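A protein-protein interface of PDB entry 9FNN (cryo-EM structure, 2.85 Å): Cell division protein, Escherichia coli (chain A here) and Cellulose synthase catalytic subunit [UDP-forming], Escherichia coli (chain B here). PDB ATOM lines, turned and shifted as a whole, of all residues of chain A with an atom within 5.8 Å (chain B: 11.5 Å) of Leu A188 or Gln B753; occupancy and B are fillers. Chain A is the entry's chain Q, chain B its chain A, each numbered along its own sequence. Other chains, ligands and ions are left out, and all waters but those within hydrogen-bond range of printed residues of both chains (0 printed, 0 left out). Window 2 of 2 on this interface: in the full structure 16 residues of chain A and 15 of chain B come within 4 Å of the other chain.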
ATOM      1  N   ILE A 183     -13.202  -8.344 -19.031  1.00  0.00           N
ATOM      2  CA  ILE A 183     -12.719  -7.347 -18.083  1.00  0.00           C
ATOM      3  C   ILE A 183     -12.879  -7.844 -16.652  1.00  0.00           C
ATOM      4  O   ILE A 183     -12.021  -7.596 -15.797  1.00  0.00           O
ATOM      5  CB  ILE A 183     -13.436  -6.004 -18.310  1.00  0.00           C
ATOM      6  CG1 ILE A 183     -13.085  -5.449 -19.688  1.00  0.00           C
ATOM      7  CG2 ILE A 183     -13.054  -5.005 -17.246  1.00  0.00           C
ATOM      8  CD1 ILE A 183     -13.768  -4.152 -20.013  1.00  0.00           C
ATOM      9  N   TYR A 184     -13.967  -8.557 -16.366  1.00  0.00           N
ATOM     10  CA  TYR A 184     -14.164  -9.094 -15.024  1.00  0.00           C
ATOM     11  C   TYR A 184     -13.142 -10.179 -14.710  1.00  0.00           C
ATOM     12  O   TYR A 184     -12.649 -10.265 -13.579  1.00  0.00           O
ATOM     13  CB  TYR A 184     -15.589  -9.624 -14.883  1.00  0.00           C
ATOM     14  CG  TYR A 184     -15.974  -9.991 -13.473  1.00  0.00           C
ATOM     15  CD1 TYR A 184     -15.985  -9.041 -12.468  1.00  0.00           C
ATOM     16  CD2 TYR A 184     -16.344 -11.286 -13.153  1.00  0.00           C
ATOM     17  CE1 TYR A 184     -16.338  -9.372 -11.182  1.00  0.00           C
ATOM     18  CE2 TYR A 184     -16.699 -11.626 -11.870  1.00  0.00           C
ATOM     19  CZ  TYR A 184     -16.693 -10.664 -10.888  1.00  0.00           C
ATOM     20  OH  TYR A 184     -17.047 -10.995  -9.603  1.00  0.00           O
ATOM     21  N   GLN A 185     -12.811 -11.017 -15.696  1.00  0.00           N
ATOM     22  CA  GLN A 185     -11.751 -12.000 -15.501  1.00  0.00           C
ATOM     23  C   GLN A 185     -10.427 -11.320 -15.197  1.00  0.00           C
ATOM     24  O   GLN A 185      -9.680 -11.765 -14.318  1.00  0.00           O
ATOM     25  CB  GLN A 185     -11.612 -12.887 -16.736  1.00  0.00           C
ATOM     26  CG  GLN A 185     -12.550 -14.064 -16.763  1.00  0.00           C
ATOM     27  CD  GLN A 185     -12.346 -14.934 -17.981  1.00  0.00           C
ATOM     28  OE1 GLN A 185     -11.627 -14.563 -18.908  1.00  0.00           O
ATOM     29  NE2 GLN A 185     -12.978 -16.101 -17.988  1.00  0.00           N
ATOM     30  N   LEU A 186     -10.115 -10.241 -15.915  1.00  0.00           N
ATOM     31  CA  LEU A 186      -8.887  -9.511 -15.623  1.00  0.00           C
ATOM     32  C   LEU A 186      -8.920  -8.901 -14.229  1.00  0.00           C
ATOM     33  O   LEU A 186      -7.907  -8.897 -13.524  1.00  0.00           O
ATOM     34  CB  LEU A 186      -8.641  -8.425 -16.667  1.00  0.00           C
ATOM     35  CG  LEU A 186      -7.673  -8.823 -17.772  1.00  0.00           C
ATOM     36  CD1 LEU A 186      -8.333  -9.821 -18.709  1.00  0.00           C
ATOM     37  CD2 LEU A 186      -7.193  -7.599 -18.524  1.00  0.00           C
ATOM     38  N   TRP A 187     -10.072  -8.369 -13.819  1.00  0.00           N
ATOM     39  CA  TRP A 187     -10.163  -7.708 -12.523  1.00  0.00           C
ATOM     40  C   TRP A 187     -10.084  -8.695 -11.370  1.00  0.00           C
ATOM     41  O   TRP A 187      -9.599  -8.343 -10.289  1.00  0.00           O
ATOM     42  CB  TRP A 187     -11.458  -6.908 -12.429  1.00  0.00           C
ATOM     43  CG  TRP A 187     -11.459  -5.666 -13.240  1.00  0.00           C
ATOM     44  CD1 TRP A 187     -10.473  -5.228 -14.065  1.00  0.00           C
ATOM     45  CD2 TRP A 187     -12.498  -4.686 -13.300  1.00  0.00           C
ATOM     46  NE1 TRP A 187     -10.832  -4.038 -14.642  1.00  0.00           N
ATOM     47  CE2 TRP A 187     -12.073  -3.684 -14.186  1.00  0.00           C
ATOM     48  CE3 TRP A 187     -13.748  -4.563 -12.691  1.00  0.00           C
ATOM     49  CZ2 TRP A 187     -12.854  -2.572 -14.480  1.00  0.00           C
ATOM     50  CZ3 TRP A 187     -14.519  -3.461 -12.983  1.00  0.00           C
ATOM     51  CH2 TRP A 187     -14.071  -2.479 -13.869  1.00  0.00           C
ATOM     52  N   LEU A 188     -10.566  -9.923 -11.568  1.00  0.00           N
ATOM     53  CA  LEU A 188     -10.496 -10.925 -10.511  1.00  0.00           C
ATOM     54  C   LEU A 188      -9.063 -11.228 -10.101  1.00  0.00           C
ATOM     55  O   LEU A 188      -8.837 -11.690  -8.976  1.00  0.00           O
ATOM     56  CB  LEU A 188     -11.194 -12.210 -10.951  1.00  0.00           C
ATOM     57  CG  LEU A 188     -12.719 -12.176 -11.041  1.00  0.00           C
ATOM     58  CD1 LEU A 188     -13.252 -13.523 -11.483  1.00  0.00           C
ATOM     59  CD2 LEU A 188     -13.318 -11.774  -9.713  1.00  0.00           C
ATOM     60  N   GLN A 189      -8.095 -10.979 -10.976  1.00  0.00           N
ATOM     61  CA  GLN A 189      -6.684 -11.181 -10.675  1.00  0.00           C
ATOM     62  C   GLN A 189      -5.924  -9.890 -10.433  1.00  0.00           C
ATOM     63  O   GLN A 189      -5.127  -9.816  -9.497  1.00  0.00           O
ATOM     64  CB  GLN A 189      -6.009 -11.951 -11.812  1.00  0.00           C
ATOM     65  CG  GLN A 189      -6.532 -13.361 -11.995  1.00  0.00           C
ATOM     66  CD  GLN A 189      -5.593 -14.226 -12.810  1.00  0.00           C
ATOM     67  OE1 GLN A 189      -4.887 -13.736 -13.691  1.00  0.00           O
ATOM     68  NE2 GLN A 189      -5.569 -15.519 -12.509  1.00  0.00           N
ATOM     69  N   SER A 190      -6.154  -8.865 -11.252  1.00  0.00           N
ATOM     70  CA  SER A 190      -5.404  -7.622 -11.140  1.00  0.00           C
ATOM     71  C   SER A 190      -5.873  -6.753  -9.982  1.00  0.00           C
ATOM     72  O   SER A 190      -5.052  -6.079  -9.352  1.00  0.00           O
ATOM     73  CB  SER A 190      -5.501  -6.839 -12.449  1.00  0.00           C
ATOM     74  OG  SER A 190      -5.026  -7.612 -13.537  1.00  0.00           O
ATOM     75  N   GLN A 191      -7.168  -6.746  -9.687  1.00  0.00           N
ATOM     76  CA  GLN A 191      -7.732  -5.866  -8.671  1.00  0.00           C
ATOM     77  C   GLN A 191      -7.833  -6.604  -7.347  1.00  0.00           C
ATOM     78  O   GLN A 191      -8.432  -7.682  -7.272  1.00  0.00           O
ATOM     79  CB  GLN A 191      -9.106  -5.350  -9.095  1.00  0.00           C
ATOM     80  CG  GLN A 191      -9.090  -4.505 -10.353  1.00  0.00           C
ATOM     81  CD  GLN A 191      -8.272  -3.243 -10.198  1.00  0.00           C
ATOM     82  OE1 GLN A 191      -8.193  -2.671  -9.112  1.00  0.00           O
ATOM     83  NE2 GLN A 191      -7.654  -2.802 -11.285  1.00  0.00           N
ATOM     84  N   ARG A 192      -7.244  -6.021  -6.304  1.00  0.00           N
ATOM     85  CA  ARG A 192      -7.231  -6.635  -4.985  1.00  0.00           C
ATOM     86  C   ARG A 192      -8.290  -6.071  -4.052  1.00  0.00           C
ATOM     87  O   ARG A 192      -8.681  -6.755  -3.100  1.00  0.00           O
ATOM     88  CB  ARG A 192      -5.854  -6.467  -4.335  1.00  0.00           C
ATOM     89  CG  ARG A 192      -4.709  -7.010  -5.168  1.00  0.00           C
ATOM     90  CD  ARG A 192      -4.896  -8.488  -5.469  1.00  0.00           C
ATOM     91  NE  ARG A 192      -3.798  -9.022  -6.264  1.00  0.00           N
ATOM     92  CZ  ARG A 192      -3.702 -10.285  -6.658  1.00  0.00           C
ATOM     93  NH1 ARG A 192      -4.627 -11.178  -6.347  1.00  0.00           N
ATOM     94  NH2 ARG A 192      -2.652 -10.660  -7.383  1.00  0.00           N
ATOM     95  N   LEU A 194     -11.328  -5.421  -4.946  1.00  0.00           N
ATOM     96  CA  LEU A 194     -12.636  -5.768  -5.479  1.00  0.00           C
ATOM     97  C   LEU A 194     -13.445  -6.534  -4.440  1.00  0.00           C
ATOM     98  O   LEU A 194     -12.967  -7.517  -3.867  1.00  0.00           O
ATOM     99  CB  LEU A 194     -12.468  -6.604  -6.747  1.00  0.00           C
ATOM    100  CG  LEU A 194     -13.599  -6.636  -7.771  1.00  0.00           C
ATOM    101  CD1 LEU A 194     -13.743  -5.290  -8.443  1.00  0.00           C
ATOM    102  CD2 LEU A 194     -13.340  -7.717  -8.799  1.00  0.00           C
ATOM    103  N   PRO A 196     -16.328  -9.106  -3.090  1.00  0.00           N
ATOM    104  CA  PRO A 196     -16.807 -10.381  -3.642  1.00  0.00           C
ATOM    105  C   PRO A 196     -18.247 -10.343  -4.121  1.00  0.00           C
ATOM    106  O   PRO A 196     -18.706 -11.326  -4.716  1.00  0.00           O
ATOM    107  CB  PRO A 196     -16.647 -11.347  -2.465  1.00  0.00           C
ATOM    108  CG  PRO A 196     -16.796 -10.478  -1.268  1.00  0.00           C
ATOM    109  CD  PRO A 196     -16.167  -9.165  -1.627  1.00  0.00           C
ATOM    110  N   MET A 197     -18.971  -9.255  -3.883  1.00  0.00           N
ATOM    111  CA  MET A 197     -20.369  -9.132  -4.265  1.00  0.00           C
ATOM    112  C   MET A 197     -20.524  -8.048  -5.319  1.00  0.00           C
ATOM    113  O   MET A 197     -19.840  -7.021  -5.274  1.00  0.00           O
ATOM    114  CB  MET A 197     -21.234  -8.812  -3.046  1.00  0.00           C
ATOM    115  CG  MET A 197     -20.784  -7.584  -2.286  1.00  0.00           C
ATOM    116  SD  MET A 197     -21.084  -7.703  -0.516  1.00  0.00           S
ATOM    117  CE  MET A 197     -20.065  -9.114  -0.099  1.00  0.00           C
ATOM    118  N   LEU A 198     -21.421  -8.280  -6.275  1.00  0.00           N
ATOM    119  CA  LEU A 198     -21.672  -7.326  -7.341  1.00  0.00           C
ATOM    120  C   LEU A 198     -23.170  -7.161  -7.541  1.00  0.00           C
ATOM    121  O   LEU A 198     -23.945  -8.103  -7.360  1.00  0.00           O
ATOM    122  CB  LEU A 198     -20.999  -7.757  -8.653  1.00  0.00           C
ATOM    123  CG  LEU A 198     -21.135  -9.200  -9.138  1.00  0.00           C
ATOM    124  CD1 LEU A 198     -22.444  -9.430  -9.863  1.00  0.00           C
ATOM    125  CD2 LEU A 198     -19.970  -9.553 -10.036  1.00  0.00           C
ATOM    126  N   ARG B 367     -13.397 -31.449 -13.687  1.00  0.00           N
ATOM    127  CA  ARG B 367     -12.278 -30.701 -14.241  1.00  0.00           C
ATOM    128  C   ARG B 367     -10.985 -30.927 -13.471  1.00  0.00           C
ATOM    129  O   ARG B 367      -9.905 -30.662 -14.006  1.00  0.00           O
ATOM    130  CB  ARG B 367     -12.614 -29.213 -14.276  1.00  0.00           C
ATOM    131  CG  ARG B 367     -13.006 -28.632 -12.933  1.00  0.00           C
ATOM    132  CD  ARG B 367     -13.635 -27.265 -13.105  1.00  0.00           C
ATOM    133  NE  ARG B 367     -13.860 -26.593 -11.832  1.00  0.00           N
ATOM    134  CZ  ARG B 367     -13.050 -25.679 -11.318  1.00  0.00           C
ATOM    135  NH1 ARG B 367     -11.946 -25.306 -11.943  1.00  0.00           N
ATOM    136  NH2 ARG B 367     -13.357 -25.125 -10.151  1.00  0.00           N
ATOM    137  N   PRO B 706     -27.216 -21.498  -5.060  1.00  0.00           N
ATOM    138  CA  PRO B 706     -27.888 -20.223  -5.316  1.00  0.00           C
ATOM    139  C   PRO B 706     -27.800 -19.855  -6.786  1.00  0.00           C
ATOM    140  O   PRO B 706     -26.824 -20.163  -7.473  1.00  0.00           O
ATOM    141  CB  PRO B 706     -27.119 -19.230  -4.440  1.00  0.00           C
ATOM    142  CG  PRO B 706     -25.788 -19.853  -4.249  1.00  0.00           C
ATOM    143  CD  PRO B 706     -26.024 -21.332  -4.215  1.00  0.00           C
ATOM    144  N   LEU B 748     -29.152 -17.808 -14.357  1.00  0.00           N
ATOM    145  CA  LEU B 748     -27.808 -17.372 -14.008  1.00  0.00           C
ATOM    146  C   LEU B 748     -27.196 -18.353 -13.015  1.00  0.00           C
ATOM    147  O   LEU B 748     -27.694 -18.501 -11.894  1.00  0.00           O
ATOM    148  CB  LEU B 748     -27.830 -15.962 -13.422  1.00  0.00           C
ATOM    149  CG  LEU B 748     -28.558 -14.889 -14.231  1.00  0.00           C
ATOM    150  CD1 LEU B 748     -28.388 -13.525 -13.592  1.00  0.00           C
ATOM    151  CD2 LEU B 748     -28.068 -14.873 -15.659  1.00  0.00           C
ATOM    152  N   LEU B 749     -26.113 -19.006 -13.425  1.00  0.00           N
ATOM    153  CA  LEU B 749     -25.388 -19.956 -12.595  1.00  0.00           C
ATOM    154  C   LEU B 749     -23.956 -19.480 -12.412  1.00  0.00           C
ATOM    155  O   LEU B 749     -23.336 -18.978 -13.354  1.00  0.00           O
ATOM    156  CB  LEU B 749     -25.391 -21.354 -13.216  1.00  0.00           C
ATOM    157  CG  LEU B 749     -26.720 -22.100 -13.265  1.00  0.00           C
ATOM    158  CD1 LEU B 749     -26.544 -23.447 -13.933  1.00  0.00           C
ATOM    159  CD2 LEU B 749     -27.284 -22.265 -11.868  1.00  0.00           C
ATOM    160  N   LYS B 750     -23.434 -19.638 -11.200  1.00  0.00           N
ATOM    161  CA  LYS B 750     -22.086 -19.204 -10.864  1.00  0.00           C
ATOM    162  C   LYS B 750     -21.197 -20.409 -10.605  1.00  0.00           C
ATOM    163  O   LYS B 750     -21.545 -21.283  -9.804  1.00  0.00           O
ATOM    164  CB  LYS B 750     -22.088 -18.287  -9.643  1.00  0.00           C
ATOM    165  CG  LYS B 750     -22.794 -16.969  -9.858  1.00  0.00           C
ATOM    166  CD  LYS B 750     -22.594 -16.048  -8.674  1.00  0.00           C
ATOM    167  CE  LYS B 750     -21.124 -15.748  -8.467  1.00  0.00           C
ATOM    168  NZ  LYS B 750     -20.519 -15.099  -9.662  1.00  0.00           N
ATOM    169  N   ARG B 751     -20.055 -20.450 -11.283  1.00  0.00           N
ATOM    170  CA  ARG B 751     -18.999 -21.423 -11.023  1.00  0.00           C
ATOM    171  C   ARG B 751     -17.843 -20.652 -10.395  1.00  0.00           C
ATOM    172  O   ARG B 751     -16.991 -20.110 -11.103  1.00  0.00           O
ATOM    173  CB  ARG B 751     -18.571 -22.128 -12.305  1.00  0.00           C
ATOM    174  CG  ARG B 751     -17.581 -23.253 -12.090  1.00  0.00           C
ATOM    175  CD  ARG B 751     -16.505 -23.247 -13.159  1.00  0.00           C
ATOM    176  NE  ARG B 751     -17.070 -23.184 -14.500  1.00  0.00           N
ATOM    177  CZ  ARG B 751     -16.350 -23.125 -15.611  1.00  0.00           C
ATOM    178  NH1 ARG B 751     -15.028 -23.124 -15.579  1.00  0.00           N
ATOM    179  NH2 ARG B 751     -16.973 -23.066 -16.785  1.00  0.00           N
ATOM    180  N   GLY B 752     -17.815 -20.610  -9.069  1.00  0.00           N
ATOM    181  CA  GLY B 752     -16.852 -19.785  -8.370  1.00  0.00           C
ATOM    182  C   GLY B 752     -17.252 -18.327  -8.370  1.00  0.00           C
ATOM    183  O   GLY B 752     -18.255 -17.953  -7.756  1.00  0.00           O
ATOM    184  N   GLN B 753     -16.475 -17.488  -9.051  1.00  0.00           N
ATOM    185  CA  GLN B 753     -16.787 -16.074  -9.187  1.00  0.00           C
ATOM    186  C   GLN B 753     -17.300 -15.715 -10.573  1.00  0.00           C
ATOM    187  O   GLN B 753     -17.585 -14.542 -10.829  1.00  0.00           O
ATOM    188  CB  GLN B 753     -15.554 -15.224  -8.861  1.00  0.00           C
ATOM    189  CG  GLN B 753     -15.120 -15.284  -7.408  1.00  0.00           C
ATOM    190  CD  GLN B 753     -16.115 -14.630  -6.474  1.00  0.00           C
ATOM    191  OE1 GLN B 753     -16.831 -13.709  -6.858  1.00  0.00           O
ATOM    192  NE2 GLN B 753     -16.166 -15.107  -5.236  1.00  0.00           N
ATOM    193  N   GLN B 754     -17.433 -16.689 -11.466  1.00  0.00           N
ATOM    194  CA  GLN B 754     -17.867 -16.452 -12.834  1.00  0.00           C
ATOM    195  C   GLN B 754     -19.321 -16.865 -12.992  1.00  0.00           C
ATOM    196  O   GLN B 754     -19.714 -17.952 -12.556  1.00  0.00           O
ATOM    197  CB  GLN B 754     -16.996 -17.220 -13.826  1.00  0.00           C
ATOM    198  CG  GLN B 754     -15.582 -16.702 -13.935  1.00  0.00           C
ATOM    199  CD  GLN B 754     -14.885 -17.195 -15.182  1.00  0.00           C
ATOM    200  OE1 GLN B 754     -13.804 -16.724 -15.530  1.00  0.00           O
ATOM    201  NE2 GLN B 754     -15.501 -18.152 -15.866  1.00  0.00           N
ATOM    202  N   GLU B 755     -20.110 -16.005 -13.624  1.00  0.00           N
ATOM    203  CA  GLU B 755     -21.531 -16.239 -13.823  1.00  0.00           C
ATOM    204  C   GLU B 755     -21.797 -16.615 -15.271  1.00  0.00           C
ATOM    205  O   GLU B 755     -21.216 -16.034 -16.191  1.00  0.00           O
ATOM    206  CB  GLU B 755     -22.337 -14.997 -13.445  1.00  0.00           C
ATOM    207  CG  GLU B 755     -23.813 -15.245 -13.238  1.00  0.00           C
ATOM    208  CD  GLU B 755     -24.537 -14.006 -12.761  1.00  0.00           C
ATOM    209  OE1 GLU B 755     -24.102 -12.892 -13.115  1.00  0.00           O
ATOM    210  OE2 GLU B 755     -25.534 -14.145 -12.021  1.00  0.00           O
ATOM    211  N   TYR B 756     -22.682 -17.585 -15.470  1.00  0.00           N
ATOM    212  CA  TYR B 756     -23.038 -18.061 -16.795  1.00  0.00           C
ATOM    213  C   TYR B 756     -24.545 -17.969 -16.976  1.00  0.00           C
ATOM    214  O   TYR B 756     -25.312 -18.117 -16.022  1.00  0.00           O
ATOM    215  CB  TYR B 756     -22.566 -19.500 -17.018  1.00  0.00           C
ATOM    216  CG  TYR B 756     -21.071 -19.678 -16.915  1.00  0.00           C
ATOM    217  CD1 TYR B 756     -20.459 -19.871 -15.688  1.00  0.00           C
ATOM    218  CD2 TYR B 756     -20.272 -19.657 -18.046  1.00  0.00           C
ATOM    219  CE1 TYR B 756     -19.096 -20.033 -15.589  1.00  0.00           C
ATOM    220  CE2 TYR B 756     -18.907 -19.820 -17.957  1.00  0.00           C
ATOM    221  CZ  TYR B 756     -18.324 -20.007 -16.727  1.00  0.00           C
ATOM    222  OH  TYR B 756     -16.962 -20.170 -16.632  1.00  0.00           O
ATOM    223  N   VAL B 757     -24.963 -17.723 -18.214  1.00  0.00           N
ATOM    224  CA  VAL B 757     -26.359 -17.484 -18.552  1.00  0.00           C
ATOM    225  C   VAL B 757     -26.826 -18.588 -19.485  1.00  0.00           C
ATOM    226  O   VAL B 757     -26.145 -18.904 -20.465  1.00  0.00           O
ATOM    227  CB  VAL B 757     -26.555 -16.105 -19.207  1.00  0.00           C
ATOM    228  CG1 VAL B 757     -28.030 -15.775 -19.301  1.00  0.00           C
ATOM    229  CG2 VAL B 757     -25.803 -15.039 -18.434  1.00  0.00           C
ATOM    230  N   GLN B 787     -19.953 -27.849 -16.887  1.00  0.00           N
ATOM    231  CA  GLN B 787     -19.022 -27.416 -15.853  1.00  0.00           C
ATOM    232  C   GLN B 787     -19.724 -26.809 -14.646  1.00  0.00           C
ATOM    233  O   GLN B 787     -19.137 -26.770 -13.562  1.00  0.00           O
ATOM    234  CB  GLN B 787     -18.023 -26.414 -16.429  1.00  0.00           C
ATOM    235  CG  GLN B 787     -17.046 -27.021 -17.412  1.00  0.00           C
ATOM    236  CD  GLN B 787     -16.173 -28.077 -16.778  1.00  0.00           C
ATOM    237  OE1 GLN B 787     -15.795 -27.966 -15.614  1.00  0.00           O
ATOM    238  NE2 GLN B 787     -15.850 -29.114 -17.540  1.00  0.00           N
ATOM    239  N   CYS B 788     -20.957 -26.329 -14.805  1.00  0.00           N
ATOM    240  CA  CYS B 788     -21.689 -25.740 -13.691  1.00  0.00           C
ATOM    241  C   CYS B 788     -22.632 -26.711 -12.998  1.00  0.00           C
ATOM    242  O   CYS B 788     -23.040 -26.440 -11.865  1.00  0.00           O
ATOM    243  CB  CYS B 788     -22.496 -24.523 -14.162  1.00  0.00           C
ATOM    244  SG  CYS B 788     -21.498 -23.094 -14.613  1.00  0.00           S
ATOM    245  N   ARG B 792     -18.776 -30.715 -11.658  1.00  0.00           N
ATOM    246  CA  ARG B 792     -18.316 -29.961 -10.502  1.00  0.00           C
ATOM    247  C   ARG B 792     -17.570 -30.907  -9.577  1.00  0.00           C
ATOM    248  O   ARG B 792     -18.076 -31.985  -9.249  1.00  0.00           O
ATOM    249  CB  ARG B 792     -19.479 -29.321  -9.748  1.00  0.00           C
ATOM    250  CG  ARG B 792     -20.253 -28.288 -10.520  1.00  0.00           C
ATOM    251  CD  ARG B 792     -21.235 -27.599  -9.601  1.00  0.00           C
ATOM    252  NE  ARG B 792     -20.562 -26.767  -8.614  1.00  0.00           N
ATOM    253  CZ  ARG B 792     -21.153 -26.249  -7.548  1.00  0.00           C
ATOM    254  NH1 ARG B 792     -22.427 -26.480  -7.285  1.00  0.00           N
ATOM    255  NH2 ARG B 792     -20.446 -25.484  -6.721  1.00  0.00           N
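Leu A188 touches one residue of chain B.
Gln B753 touches three residues of chain A.
Tyr A184 touches just one residue of chain B: Gln B753.
No residue of chain B comes within 4 Å of Gln A189.
No residue of chain B comes within 4 Å of Ser A190.
Of the printed residues of chain A, Gln B754 touches Gln A185.
Of the printed residues of chain B, Gln A185 touches Gln B754.
The nearest residue of chain A that does not touch Gln B753 is Leu A198 (5.6 Å).
The side-chain amide nitrogen (NE2) of Gln A185 is in hydrogen-bond range of the side-chain amide oxygen (OE1) of Gln B754, at 2.7 Å.
The side-chain amino group (NZ) of Lys B750 is in hydrogen-bond range of the backbone carbonyl oxygen (O) of Gln B753 (3.2 Å).
The side-chain amide nitrogen of Gln B754 is in hydrogen-bond range of the side-chain hydroxyl of Tyr B756, at 2.6 Å.
Of the 14 printed residues of chain A, 4 touch a printed residue of chain B.
Among the printed residues, 4 pairs touch across the chains.
Among the printed residues, merely in contact across the chains: Tyr A184 with Gln B753, Pro A196 with Gln B753 and Leu A188 with Gln B753.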
